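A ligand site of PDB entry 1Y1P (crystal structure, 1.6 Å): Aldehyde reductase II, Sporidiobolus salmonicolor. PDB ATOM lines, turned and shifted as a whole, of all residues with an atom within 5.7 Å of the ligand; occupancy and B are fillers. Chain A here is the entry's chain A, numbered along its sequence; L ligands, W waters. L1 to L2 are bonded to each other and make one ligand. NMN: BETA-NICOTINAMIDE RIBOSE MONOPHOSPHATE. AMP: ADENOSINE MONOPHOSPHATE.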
ATOM      1  N   THR A  17      -0.947 -15.080 -28.345  1.00  0.00           N
ATOM      2  CA  THR A  17      -0.625 -14.186 -29.439  1.00  0.00           C
ATOM      3  C   THR A  17       0.297 -13.048 -29.013  1.00  0.00           C
ATOM      4  O   THR A  17       0.145 -12.464 -27.928  1.00  0.00           O
ATOM      5  CB  THR A  17      -1.909 -13.592 -30.080  1.00  0.00           C
ATOM      6  OG1 THR A  17      -2.562 -12.713 -29.154  1.00  0.00           O
ATOM      7  CG2 THR A  17      -2.863 -14.731 -30.451  1.00  0.00           C
ATOM      8  N   GLY A  18       1.267 -12.730 -29.874  1.00  0.00           N
ATOM      9  CA  GLY A  18       2.210 -11.672 -29.578  1.00  0.00           C
ATOM     10  C   GLY A  18       3.088 -12.085 -28.408  1.00  0.00           C
ATOM     11  O   GLY A  18       3.362 -11.285 -27.516  1.00  0.00           O
ATOM     12  N   ALA A  19       3.515 -13.350 -28.423  1.00  0.00           N
ATOM     13  CA  ALA A  19       4.348 -13.920 -27.365  1.00  0.00           C
ATOM     14  C   ALA A  19       5.700 -13.250 -27.134  1.00  0.00           C
ATOM     15  O   ALA A  19       6.333 -13.479 -26.100  1.00  0.00           O
ATOM     16  CB  ALA A  19       4.554 -15.413 -27.626  1.00  0.00           C
ATOM     17  N   ASN A  20       6.155 -12.435 -28.087  1.00  0.00           N
ATOM     18  CA  ASN A  20       7.441 -11.747 -27.934  1.00  0.00           C
ATOM     19  C   ASN A  20       7.282 -10.470 -27.125  1.00  0.00           C
ATOM     20  O   ASN A  20       8.269  -9.832 -26.759  1.00  0.00           O
ATOM     21  CB  ASN A  20       8.035 -11.415 -29.305  1.00  0.00           C
ATOM     22  CG  ASN A  20       7.192 -10.420 -30.069  1.00  0.00           C
ATOM     23  OD1 ASN A  20       6.004 -10.637 -30.297  1.00  0.00           O
ATOM     24  ND2 ASN A  20       7.812  -9.309 -30.476  1.00  0.00           N
ATOM     25  N   GLY A  21       6.042 -10.105 -26.835  1.00  0.00           N
ATOM     26  CA  GLY A  21       5.771  -8.894 -26.063  1.00  0.00           C
ATOM     27  C   GLY A  21       6.140  -9.063 -24.599  1.00  0.00           C
ATOM     28  O   GLY A  21       6.333 -10.184 -24.127  1.00  0.00           O
ATOM     29  N   PHE A  22       6.239  -7.952 -23.885  1.00  0.00           N
ATOM     30  CA  PHE A  22       6.603  -7.990 -22.468  1.00  0.00           C
ATOM     31  C   PHE A  22       5.594  -8.756 -21.609  1.00  0.00           C
ATOM     32  O   PHE A  22       5.931  -9.767 -21.003  1.00  0.00           O
ATOM     33  CB  PHE A  22       6.782  -6.560 -21.947  1.00  0.00           C
ATOM     34  CG  PHE A  22       7.031  -6.469 -20.466  1.00  0.00           C
ATOM     35  CD1 PHE A  22       8.155  -7.060 -19.904  1.00  0.00           C
ATOM     36  CD2 PHE A  22       6.118  -5.829 -19.632  1.00  0.00           C
ATOM     37  CE1 PHE A  22       8.380  -7.015 -18.519  1.00  0.00           C
ATOM     38  CE2 PHE A  22       6.338  -5.775 -18.257  1.00  0.00           C
ATOM     39  CZ  PHE A  22       7.462  -6.366 -17.696  1.00  0.00           C
ATOM     40  N   VAL A  23       4.348  -8.272 -21.554  1.00  0.00           N
ATOM     41  CA  VAL A  23       3.331  -8.942 -20.764  1.00  0.00           C
ATOM     42  C   VAL A  23       3.137 -10.379 -21.223  1.00  0.00           C
ATOM     43  O   VAL A  23       3.076 -11.311 -20.409  1.00  0.00           O
ATOM     44  CB  VAL A  23       1.990  -8.176 -20.827  1.00  0.00           C
ATOM     45  CG1 VAL A  23       0.879  -9.008 -20.203  1.00  0.00           C
ATOM     46  CG2 VAL A  23       2.126  -6.831 -20.120  1.00  0.00           C
ATOM     47  N   ALA A  24       3.039 -10.572 -22.539  1.00  0.00           N
ATOM     48  CA  ALA A  24       2.846 -11.907 -23.086  1.00  0.00           C
ATOM     49  C   ALA A  24       3.945 -12.884 -22.661  1.00  0.00           C
ATOM     50  O   ALA A  24       3.648 -14.028 -22.309  1.00  0.00           O
ATOM     51  CB  ALA A  24       2.765 -11.835 -24.599  1.00  0.00           C
ATOM     52  N   ARG A  43       5.167 -11.682 -35.201  1.00  0.00           N
ATOM     53  CA  ARG A  43       5.126 -11.302 -36.598  1.00  0.00           C
ATOM     54  C   ARG A  43       6.310 -11.859 -37.392  1.00  0.00           C
ATOM     55  O   ARG A  43       6.323 -11.802 -38.631  1.00  0.00           O
ATOM     56  CB  ARG A  43       4.985  -9.792 -36.736  1.00  0.00           C
ATOM     57  CG  ARG A  43       3.594  -9.342 -36.294  1.00  0.00           C
ATOM     58  CD  ARG A  43       3.241  -7.948 -36.749  1.00  0.00           C
ATOM     59  NE  ARG A  43       3.789  -6.923 -35.877  1.00  0.00           N
ATOM     60  CZ  ARG A  43       3.607  -5.620 -36.063  1.00  0.00           C
ATOM     61  NH1 ARG A  43       2.901  -5.188 -37.105  1.00  0.00           N
ATOM     62  NH2 ARG A  43       4.122  -4.747 -35.209  1.00  0.00           N
ATOM     63  N   LYS A  47      11.807 -12.431 -34.069  1.00  0.00           N
ATOM     64  CA  LYS A  47      11.374 -11.666 -32.907  1.00  0.00           C
ATOM     65  C   LYS A  47      11.263 -12.517 -31.649  1.00  0.00           C
ATOM     66  O   LYS A  47      11.362 -12.016 -30.531  1.00  0.00           O
ATOM     67  CB  LYS A  47      10.038 -10.970 -33.196  1.00  0.00           C
ATOM     68  CG  LYS A  47      10.182  -9.705 -34.046  1.00  0.00           C
ATOM     69  CD  LYS A  47       8.843  -9.094 -34.406  1.00  0.00           C
ATOM     70  CE  LYS A  47       9.025  -7.801 -35.183  1.00  0.00           C
ATOM     71  NZ  LYS A  47       7.739  -7.230 -35.659  1.00  0.00           N
ATOM     72  N   GLU A  69       2.289 -13.070 -39.306  1.00  0.00           N
ATOM     73  CA  GLU A  69       2.719 -11.749 -39.734  1.00  0.00           C
ATOM     74  C   GLU A  69       1.633 -10.682 -39.723  1.00  0.00           C
ATOM     75  O   GLU A  69       1.915  -9.504 -39.526  1.00  0.00           O
ATOM     76  CB  GLU A  69       3.337 -11.840 -41.132  1.00  0.00           C
ATOM     77  CG  GLU A  69       4.363 -12.948 -41.259  1.00  0.00           C
ATOM     78  CD  GLU A  69       4.949 -13.059 -42.653  1.00  0.00           C
ATOM     79  OE1 GLU A  69       4.180 -13.048 -43.641  1.00  0.00           O
ATOM     80  OE2 GLU A  69       6.192 -13.189 -42.768  1.00  0.00           O
ATOM     81  N   MET A  71      -2.039 -10.159 -37.917  1.00  0.00           N
ATOM     82  CA  MET A  71      -3.088 -10.632 -37.014  1.00  0.00           C
ATOM     83  C   MET A  71      -4.498 -10.269 -37.438  1.00  0.00           C
ATOM     84  O   MET A  71      -5.470 -10.692 -36.812  1.00  0.00           O
ATOM     85  CB  MET A  71      -2.838 -10.129 -35.579  1.00  0.00           C
ATOM     86  CG  MET A  71      -3.142  -8.662 -35.352  1.00  0.00           C
ATOM     87  SD  MET A  71      -3.018  -8.204 -33.591  1.00  0.00           S
ATOM     88  CE  MET A  71      -3.431  -6.461 -33.689  1.00  0.00           C
ATOM     89  N   ILE A  90      -3.087 -11.427 -26.529  1.00  0.00           N
ATOM     90  CA  ILE A  90      -2.383 -10.343 -25.868  1.00  0.00           C
ATOM     91  C   ILE A  90      -1.910  -9.217 -26.796  1.00  0.00           C
ATOM     92  O   ILE A  90      -1.842  -8.057 -26.373  1.00  0.00           O
ATOM     93  CB  ILE A  90      -1.178 -10.920 -25.091  1.00  0.00           C
ATOM     94  CG1 ILE A  90      -1.648 -12.116 -24.264  1.00  0.00           C
ATOM     95  CG2 ILE A  90      -0.554  -9.853 -24.203  1.00  0.00           C
ATOM     96  CD1 ILE A  90      -0.593 -12.733 -23.365  1.00  0.00           C
ATOM     97  N   ALA A  91      -1.588  -9.563 -28.029  1.00  0.00           N
ATOM     98  CA  ALA A  91      -1.112  -8.569 -28.992  1.00  0.00           C
ATOM     99  C   ALA A  91      -2.113  -7.453 -29.285  1.00  0.00           C
ATOM    100  O   ALA A  91      -3.292  -7.712 -29.486  1.00  0.00           O
ATOM    101  CB  ALA A  91      -0.735  -9.264 -30.299  1.00  0.00           C
ATOM    102  N   SER A  92      -1.622  -6.219 -29.295  1.00  0.00           N
ATOM    103  CA  SER A  92      -2.450  -5.054 -29.589  1.00  0.00           C
ATOM    104  C   SER A  92      -1.531  -3.892 -29.969  1.00  0.00           C
ATOM    105  O   SER A  92      -0.332  -3.933 -29.707  1.00  0.00           O
ATOM    106  CB  SER A  92      -3.308  -4.668 -28.384  1.00  0.00           C
ATOM    107  OG  SER A  92      -4.302  -3.713 -28.755  1.00  0.00           O
ATOM    108  N   VAL A  93      -2.095  -2.859 -30.606  1.00  0.00           N
ATOM    109  CA  VAL A  93      -1.314  -1.702 -31.042  1.00  0.00           C
ATOM    110  C   VAL A  93      -0.835  -0.849 -29.870  1.00  0.00           C
ATOM    111  O   VAL A  93      -1.648  -0.296 -29.116  1.00  0.00           O
ATOM    112  CB  VAL A  93      -2.134  -0.821 -32.001  1.00  0.00           C
ATOM    113  CG1 VAL A  93      -1.294   0.364 -32.478  1.00  0.00           C
ATOM    114  CG2 VAL A  93      -2.613  -1.651 -33.182  1.00  0.00           C
ATOM    115  N   VAL A  94       0.476  -0.740 -29.741  1.00  0.00           N
ATOM    116  CA  VAL A  94       1.086   0.039 -28.660  1.00  0.00           C
ATOM    117  C   VAL A  94       2.077   1.068 -29.202  1.00  0.00           C
ATOM    118  O   VAL A  94       3.045   1.413 -28.540  1.00  0.00           O
ATOM    119  CB  VAL A  94       1.822  -0.890 -27.668  1.00  0.00           C
ATOM    120  CG1 VAL A  94       0.828  -1.821 -26.998  1.00  0.00           C
ATOM    121  CG2 VAL A  94       2.892  -1.689 -28.406  1.00  0.00           C
ATOM    122  N   PRO A 106      -7.563  -1.486 -35.792  1.00  0.00           N
ATOM    123  CA  PRO A 106      -6.789  -2.733 -35.730  1.00  0.00           C
ATOM    124  C   PRO A 106      -6.930  -3.454 -34.393  1.00  0.00           C
ATOM    125  O   PRO A 106      -6.939  -4.680 -34.347  1.00  0.00           O
ATOM    126  CB  PRO A 106      -5.350  -2.258 -35.968  1.00  0.00           C
ATOM    127  CG  PRO A 106      -5.545  -1.055 -36.836  1.00  0.00           C
ATOM    128  CD  PRO A 106      -6.684  -0.357 -36.154  1.00  0.00           C
ATOM    129  N   THR A 130      -6.248  -9.822 -23.041  1.00  0.00           N
ATOM    130  CA  THR A 130      -5.486  -8.844 -22.271  1.00  0.00           C
ATOM    131  C   THR A 130      -6.029  -7.462 -22.619  1.00  0.00           C
ATOM    132  O   THR A 130      -5.844  -6.969 -23.740  1.00  0.00           O
ATOM    133  CB  THR A 130      -3.981  -8.876 -22.606  1.00  0.00           C
ATOM    134  OG1 THR A 130      -3.467 -10.202 -22.429  1.00  0.00           O
ATOM    135  CG2 THR A 130      -3.222  -7.912 -21.694  1.00  0.00           C
ATOM    136  N   SER A 131      -6.742  -6.870 -21.674  1.00  0.00           N
ATOM    137  CA  SER A 131      -7.305  -5.537 -21.832  1.00  0.00           C
ATOM    138  C   SER A 131      -6.369  -4.609 -21.035  1.00  0.00           C
ATOM    139  O   SER A 131      -5.154  -4.788 -21.059  1.00  0.00           O
ATOM    140  CB  SER A 131      -8.730  -5.507 -21.265  1.00  0.00           C
ATOM    141  OG  SER A 131      -9.350  -4.238 -21.417  1.00  0.00           O
ATOM    142  N   SER A 132      -6.940  -3.633 -20.332  1.00  0.00           N
ATOM    143  CA  SER A 132      -6.142  -2.697 -19.547  1.00  0.00           C
ATOM    144  C   SER A 132      -7.045  -1.879 -18.638  1.00  0.00           C
ATOM    145  O   SER A 132      -8.263  -1.804 -18.880  1.00  0.00           O
ATOM    146  CB  SER A 132      -5.390  -1.734 -20.471  1.00  0.00           C
ATOM    147  OG  SER A 132      -4.785  -0.667 -19.740  1.00  0.00           O
ATOM    148  N   THR A 133      -6.481  -1.300 -17.585  1.00  0.00           N
ATOM    149  CA  THR A 133      -7.277  -0.463 -16.706  1.00  0.00           C
ATOM    150  C   THR A 133      -7.778   0.745 -17.503  1.00  0.00           C
ATOM    151  O   THR A 133      -8.754   1.377 -17.105  1.00  0.00           O
ATOM    152  CB  THR A 133      -6.482   0.033 -15.476  1.00  0.00           C
ATOM    153  OG1 THR A 133      -5.188   0.527 -15.879  1.00  0.00           O
ATOM    154  CG2 THR A 133      -6.299  -1.092 -14.474  1.00  0.00           C
ATOM    155  N   TYR A 176      -5.273   5.428 -27.407  1.00  0.00           N
ATOM    156  CA  TYR A 176      -4.925   4.095 -26.943  1.00  0.00           C
ATOM    157  C   TYR A 176      -6.036   3.581 -26.030  1.00  0.00           C
ATOM    158  O   TYR A 176      -6.485   2.446 -26.161  1.00  0.00           O
ATOM    159  CB  TYR A 176      -3.579   4.129 -26.196  1.00  0.00           C
ATOM    160  CG  TYR A 176      -3.256   2.868 -25.422  1.00  0.00           C
ATOM    161  CD1 TYR A 176      -3.326   2.850 -24.026  1.00  0.00           C
ATOM    162  CD2 TYR A 176      -2.850   1.703 -26.067  1.00  0.00           C
ATOM    163  CE1 TYR A 176      -3.013   1.706 -23.299  1.00  0.00           C
ATOM    164  CE2 TYR A 176      -2.541   0.539 -25.348  1.00  0.00           C
ATOM    165  CZ  TYR A 176      -2.620   0.554 -23.957  1.00  0.00           C
ATOM    166  OH  TYR A 176      -2.324  -0.591 -23.244  1.00  0.00           O
ATOM    167  N   LYS A 180      -8.389   0.158 -26.479  1.00  0.00           N
ATOM    168  CA  LYS A 180      -8.546  -0.916 -25.510  1.00  0.00           C
ATOM    169  C   LYS A 180     -10.018  -1.061 -25.123  1.00  0.00           C
ATOM    170  O   LYS A 180     -10.547  -2.173 -25.081  1.00  0.00           O
ATOM    171  CB  LYS A 180      -7.695  -0.639 -24.270  1.00  0.00           C
ATOM    172  CG  LYS A 180      -6.197  -0.560 -24.546  1.00  0.00           C
ATOM    173  CD  LYS A 180      -5.673  -1.844 -25.195  1.00  0.00           C
ATOM    174  CE  LYS A 180      -5.797  -3.046 -24.252  1.00  0.00           C
ATOM    175  NZ  LYS A 180      -5.305  -4.298 -24.876  1.00  0.00           N
ATOM    176  N   LEU A 204      -7.147  -6.979 -16.837  1.00  0.00           N
ATOM    177  CA  LEU A 204      -6.932  -5.542 -17.032  1.00  0.00           C
ATOM    178  C   LEU A 204      -5.791  -5.033 -16.176  1.00  0.00           C
ATOM    179  O   LEU A 204      -5.992  -4.539 -15.073  1.00  0.00           O
ATOM    180  CB  LEU A 204      -8.223  -4.777 -16.693  1.00  0.00           C
ATOM    181  CG  LEU A 204      -9.371  -4.830 -17.714  1.00  0.00           C
ATOM    182  CD1 LEU A 204      -9.924  -6.251 -17.858  1.00  0.00           C
ATOM    183  CD2 LEU A 204     -10.460  -3.884 -17.240  1.00  0.00           C
ATOM    184  N   PRO A 205      -4.551  -5.141 -16.683  1.00  0.00           N
ATOM    185  CA  PRO A 205      -3.403  -4.666 -15.905  1.00  0.00           C
ATOM    186  C   PRO A 205      -3.282  -3.143 -15.921  1.00  0.00           C
ATOM    187  O   PRO A 205      -3.792  -2.483 -16.831  1.00  0.00           O
ATOM    188  CB  PRO A 205      -2.206  -5.291 -16.616  1.00  0.00           C
ATOM    189  CG  PRO A 205      -2.807  -6.373 -17.518  1.00  0.00           C
ATOM    190  CD  PRO A 205      -4.108  -5.778 -17.932  1.00  0.00           C
ATOM    191  N   ASN A 206      -2.632  -2.604 -14.894  1.00  0.00           N
ATOM    192  CA  ASN A 206      -2.332  -1.184 -14.885  1.00  0.00           C
ATOM    193  C   ASN A 206      -0.836  -1.205 -15.217  1.00  0.00           C
ATOM    194  O   ASN A 206      -0.426  -1.957 -16.095  1.00  0.00           O
ATOM    195  CB  ASN A 206      -2.615  -0.522 -13.529  1.00  0.00           C
ATOM    196  CG  ASN A 206      -2.739   1.010 -13.632  1.00  0.00           C
ATOM    197  OD1 ASN A 206      -3.326   1.648 -12.773  1.00  0.00           O
ATOM    198  ND2 ASN A 206      -2.185   1.575 -14.686  1.00  0.00           N
ATOM    199  N   TYR A 207       0.005  -0.435 -14.520  1.00  0.00           N
ATOM    200  CA  TYR A 207       1.433  -0.390 -14.849  1.00  0.00           C
ATOM    201  C   TYR A 207       2.193  -1.658 -14.438  1.00  0.00           C
ATOM    202  O   TYR A 207       2.504  -1.853 -13.264  1.00  0.00           O
ATOM    203  CB  TYR A 207       2.073   0.841 -14.183  1.00  0.00           C
ATOM    204  CG  TYR A 207       3.292   1.361 -14.900  1.00  0.00           C
ATOM    205  CD1 TYR A 207       3.219   2.450 -15.748  1.00  0.00           C
ATOM    206  CD2 TYR A 207       4.531   0.740 -14.731  1.00  0.00           C
ATOM    207  CE1 TYR A 207       4.352   2.935 -16.418  1.00  0.00           C
ATOM    208  CE2 TYR A 207       5.665   1.210 -15.386  1.00  0.00           C
ATOM    209  CZ  TYR A 207       5.569   2.298 -16.235  1.00  0.00           C
ATOM    210  OH  TYR A 207       6.702   2.752 -16.873  1.00  0.00           O
ATOM    211  N   THR A 208       2.507  -2.507 -15.419  1.00  0.00           N
ATOM    212  CA  THR A 208       3.184  -3.772 -15.143  1.00  0.00           C
ATOM    213  C   THR A 208       4.705  -3.664 -15.007  1.00  0.00           C
ATOM    214  O   THR A 208       5.420  -3.283 -15.940  1.00  0.00           O
ATOM    215  CB  THR A 208       2.813  -4.805 -16.229  1.00  0.00           C
ATOM    216  OG1 THR A 208       1.376  -4.891 -16.329  1.00  0.00           O
ATOM    217  CG2 THR A 208       3.338  -6.190 -15.864  1.00  0.00           C
ATOM    218  N   SER A 219      11.614  -4.410 -26.097  1.00  0.00           N
ATOM    219  CA  SER A 219      11.732  -3.023 -25.662  1.00  0.00           C
ATOM    220  C   SER A 219      11.333  -2.909 -24.195  1.00  0.00           C
ATOM    221  O   SER A 219      11.810  -2.038 -23.482  1.00  0.00           O
ATOM    222  CB  SER A 219      10.856  -2.115 -26.537  1.00  0.00           C
ATOM    223  OG  SER A 219       9.673  -2.776 -26.972  1.00  0.00           O
ATOM    224  N   GLY A 220      10.454  -3.813 -23.748  1.00  0.00           N
ATOM    225  CA  GLY A 220      10.053  -3.791 -22.359  1.00  0.00           C
ATOM    226  C   GLY A 220       8.741  -3.100 -22.031  1.00  0.00           C
ATOM    227  O   GLY A 220       8.257  -3.246 -20.902  1.00  0.00           O
ATOM    228  N   SER A 221       8.172  -2.339 -22.961  1.00  0.00           N
ATOM    229  CA  SER A 221       6.906  -1.684 -22.667  1.00  0.00           C
ATOM    230  C   SER A 221       7.083  -0.890 -21.373  1.00  0.00           C
ATOM    231  O   SER A 221       8.114  -0.257 -21.156  1.00  0.00           O
ATOM    232  CB  SER A 221       5.780  -2.715 -22.511  1.00  0.00           C
ATOM    233  OG  SER A 221       4.509  -2.083 -22.436  1.00  0.00           O
ATOM    234  N   THR A 222       6.021  -0.848 -20.565  1.00  0.00           N
ATOM    235  CA  THR A 222       6.034  -0.157 -19.286  1.00  0.00           C
ATOM    236  C   THR A 222       7.333  -0.341 -18.491  1.00  0.00           C
ATOM    237  O   THR A 222       7.870   0.624 -17.943  1.00  0.00           O
ATOM    238  CB  THR A 222       4.865  -0.636 -18.395  1.00  0.00           C
ATOM    239  OG1 THR A 222       4.833  -2.068 -18.384  1.00  0.00           O
ATOM    240  CG2 THR A 222       3.549  -0.096 -18.939  1.00  0.00           C
HETATM  241  O3P NMN L   1       3.786  -4.166 -24.818  1.00  0.00           O
HETATM  242  P   NMN L   1       2.973  -4.986 -23.842  1.00  0.00           P
HETATM  243  O1P NMN L   1       3.478  -6.321 -23.442  1.00  0.00           O
HETATM  244  O2P NMN L   1       2.744  -3.960 -22.780  1.00  0.00           O
HETATM  245  O5R NMN L   1       1.557  -5.208 -24.542  1.00  0.00           O
HETATM  246  C5R NMN L   1       0.864  -6.449 -24.446  1.00  0.00           C
HETATM  247  C4R NMN L   1      -0.599  -6.208 -24.123  1.00  0.00           C
HETATM  248  O4R NMN L   1      -0.714  -5.832 -22.728  1.00  0.00           O
HETATM  249  C3R NMN L   1      -1.304  -5.113 -24.926  1.00  0.00           C
HETATM  250  O3R NMN L   1      -2.588  -5.571 -25.355  1.00  0.00           O
HETATM  251  C2R NMN L   1      -1.457  -3.983 -23.911  1.00  0.00           C
HETATM  252  O2R NMN L   1      -2.577  -3.158 -24.154  1.00  0.00           O
HETATM  253  C1R NMN L   1      -1.641  -4.783 -22.622  1.00  0.00           C
HETATM  254  N1  NMN L   1      -1.418  -4.054 -21.360  1.00  0.00           N
HETATM  255  C2  NMN L   1      -0.087  -3.851 -20.899  1.00  0.00           C
HETATM  256  C3  NMN L   1       0.121  -3.209 -19.735  1.00  0.00           C
HETATM  257  C7  NMN L   1       1.464  -2.982 -19.226  1.00  0.00           C
HETATM  258  O7  NMN L   1       1.599  -2.393 -18.153  1.00  0.00           O
HETATM  259  N7  NMN L   1       2.507  -3.402 -19.936  1.00  0.00           N
HETATM  260  C4  NMN L   1      -1.007  -2.748 -18.998  1.00  0.00           C
HETATM  261  C5  NMN L   1      -2.338  -2.958 -19.466  1.00  0.00           C
HETATM  262  C6  NMN L   1      -2.493  -3.610 -20.633  1.00  0.00           C
HETATM  263  P   AMP L   2       4.896  -4.764 -25.659  1.00  0.00           P
HETATM  264  O1P AMP L   2       5.975  -5.369 -24.843  1.00  0.00           O
HETATM  265  O2P AMP L   2       5.201  -3.580 -26.507  1.00  0.00           O
HETATM  266  O5' AMP L   2       4.305  -5.898 -26.607  1.00  0.00           O
HETATM  267  C5' AMP L   2       3.222  -5.637 -27.488  1.00  0.00           C
HETATM  268  C4' AMP L   2       2.994  -6.821 -28.402  1.00  0.00           C
HETATM  269  O4' AMP L   2       1.943  -6.529 -29.371  1.00  0.00           O
HETATM  270  C3' AMP L   2       4.182  -7.336 -29.198  1.00  0.00           C
HETATM  271  O3' AMP L   2       4.252  -8.751 -29.143  1.00  0.00           O
HETATM  272  C2' AMP L   2       3.915  -6.794 -30.594  1.00  0.00           C
HETATM  273  O2' AMP L   2       4.511  -7.482 -31.673  1.00  0.00           O
HETATM  274  C1' AMP L   2       2.392  -6.898 -30.663  1.00  0.00           C
HETATM  275  N9  AMP L   2       1.782  -6.003 -31.631  1.00  0.00           N
HETATM  276  C8  AMP L   2       1.756  -4.627 -31.630  1.00  0.00           C
HETATM  277  N7  AMP L   2       1.188  -4.112 -32.696  1.00  0.00           N
HETATM  278  C5  AMP L   2       0.812  -5.221 -33.449  1.00  0.00           C
HETATM  279  C6  AMP L   2       0.170  -5.349 -34.691  1.00  0.00           C
HETATM  280  N6  AMP L   2      -0.236  -4.309 -35.415  1.00  0.00           N
HETATM  281  N1  AMP L   2      -0.048  -6.599 -35.154  1.00  0.00           N
HETATM  282  C2  AMP L   2       0.354  -7.638 -34.418  1.00  0.00           C
HETATM  283  N3  AMP L   2       0.976  -7.641 -33.242  1.00  0.00           N
HETATM  284  C4  AMP L   2       1.173  -6.390 -32.809  1.00  0.00           C
HETATM  285  O   HOH W   1       2.297 -10.235 -32.810  1.00  0.00           O
HETATM  286  O   HOH W   2       0.597  -1.695 -35.203  1.00  0.00           O
HETATM  287  O   HOH W   3      -2.418   0.256 -20.133  1.00  0.00           O
HETATM  288  O   HOH W   4       5.139 -10.005 -32.828  1.00  0.00           O
HETATM  289  O   HOH W   5       1.801  -1.463 -32.257  1.00  0.00           O
HETATM  290  O   HOH W   6       1.632  -9.331 -26.899  1.00  0.00           O
HETATM  291  O   HOH W   7       7.518  -2.050 -25.765  1.00  0.00           O
HETATM  292  O   HOH W   8       4.606  -3.288 -31.049  1.00  0.00           O
HETATM  293  O   HOH W   9      -0.718  -7.549 -37.757  1.00  0.00           O
HETATM  294  O   HOH W  10       6.362  -3.377 -28.969  1.00  0.00           O
HETATM  295  O   HOH W  11       8.606  -5.748 -25.118  1.00  0.00           O
HETATM  296  O   HOH W  12       4.298  -1.395 -25.046  1.00  0.00           O
HETATM  297  O   HOH W  13       2.963  -8.599 -24.582  1.00  0.00           O
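The side-chain hydroxyl of Thr 208 is in hydrogen-bond range of an oxygen (O7) of NMN L1 (3.1 Å). An oxygen (O3R) of NMN L1 is in hydrogen-bond range of the backbone carbonyl oxygen of Ile 90, 2.8 Å away. An oxygen (O2R) of NMN L1 lies within hydrogen-bond range of the side-chain hydroxyl (OH) of Tyr 176 (2.7 Å). The backbone NH (N) of Phe 22 lies within hydrogen-bond range of an oxygen (O1P) of AMP L2, 2.8 Å away. N of Val 23 sits at hydrogen-bond distance from O1P of NMN L1 (2.9 Å). OG1 of Thr 222 sits at hydrogen-bond distance from N7 of NMN L1 (3.1 Å). The backbone carbonyl oxygen (O) of Gly 18 sits at hydrogen-bond distance from an oxygen (O3') of AMP L2 (3.1 Å). OD1 of Asn 20 lies within hydrogen-bond range of O3' of AMP L2, 2.8 Å away. The backbone NH (N) of Thr 208 is in hydrogen-bond range of an oxygen (O7) of NMN L1 (2.9 Å). OG of Ser 221 is in hydrogen-bond range of O2P of NMN L1. The side-chain amino group (NZ) of Lys 180 lies within hydrogen-bond range of an oxygen (O3R) of NMN L1, at 3.0 Å. An oxygen (O3') of AMP L2 lies within hydrogen-bond range of the backbone NH (N) of Gly 21, 3.2 Å away.
The backbone NH (N) of Ala 91 sits at hydrogen-bond distance from the backbone carbonyl oxygen (O) of Thr 17. The backbone carbonyl oxygen (O) of Thr 208 lies within hydrogen-bond range of the side-chain hydroxyl (OG1) of Thr 222 (2.8 Å). The backbone NH (N) of Ile 90 is in hydrogen-bond range of the side-chain hydroxyl (OG1) of Thr 17. OH of Tyr 207 is in hydrogen-bond range of O of Thr 222, at 2.7 Å. N of Thr 133 is in hydrogen-bond range of O of Pro 205, 3.0 Å away. O of Asn 206 lies within hydrogen-bond range of OG1 of Thr 208 (3.5 Å). ND2 of Asn 206 sits close to OG1 of Thr 133 (3.4 Å). O of Thr 130 lies within hydrogen-bond range of NZ of Lys 180 (3.0 Å).
The side-chain sulfur of Met 71 sits close to a nitrogen (N1) of AMP L2, 3.7 Å away. A nitrogen (N7) of AMP L2 sits close to the backbone carbonyl oxygen (O) of Ser 92 (3.4 Å). O of Asn 206 lies close to O7 of NMN L1 (2.9 Å). Residues that only touch the ligand: Ser 131 (2.9 Å), Pro 205 (3.0 Å), Ser 132 (3.4 Å), Thr 130 (3.4 Å), Val 94 (3.5 Å), Arg 43 (3.6 Å), Ala 91 (3.7 Å), Tyr 207 (3.8 Å) and Val 93 (3.8 Å). Hydrophobic or aromatic side chains within 4 Å of the ligand: Phe 22, Val 23, Met 71, Ile 90, Ala 91, Val 94, Tyr 176 and Pro 205. Within 4 Å of the ligand: Gly 18, Asn 20, Gly 21, Phe 22, Val 23, Arg 43, Met 71, Ile 90, Ala 91, Ser 92, Val 93, Val 94, Thr 130, Ser 131, Ser 132, Tyr 176, Lys 180, Pro 205, Asn 206, Tyr 207, Thr 208, Ser 221 and Thr 222.
Water W12 bridges the side-chain hydroxyl (OG) of Ser 221 and an oxygen (O2P) of AMP L2. Water W4 lies within hydrogen-bond range of OD1 of Asn 20 (2.7 Å), O2' of AMP L2 (2.8 Å) and N of Arg 43 (2.9 Å). Water W9 bridges N1 of AMP L2 (2.9 Å) and N of Met 71 (2.9 Å). Water W7 lies within hydrogen-bond range of OG of Ser 219, O2P of AMP L2 and N of Ser 221. Water W6 lies within hydrogen-bond range of O of Gly 18, N of Ala 91 and O3' of AMP L2. Water W3 bridges OG of Ser 132 (2.6 Å) and OH of Tyr 176 (3.2 Å).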
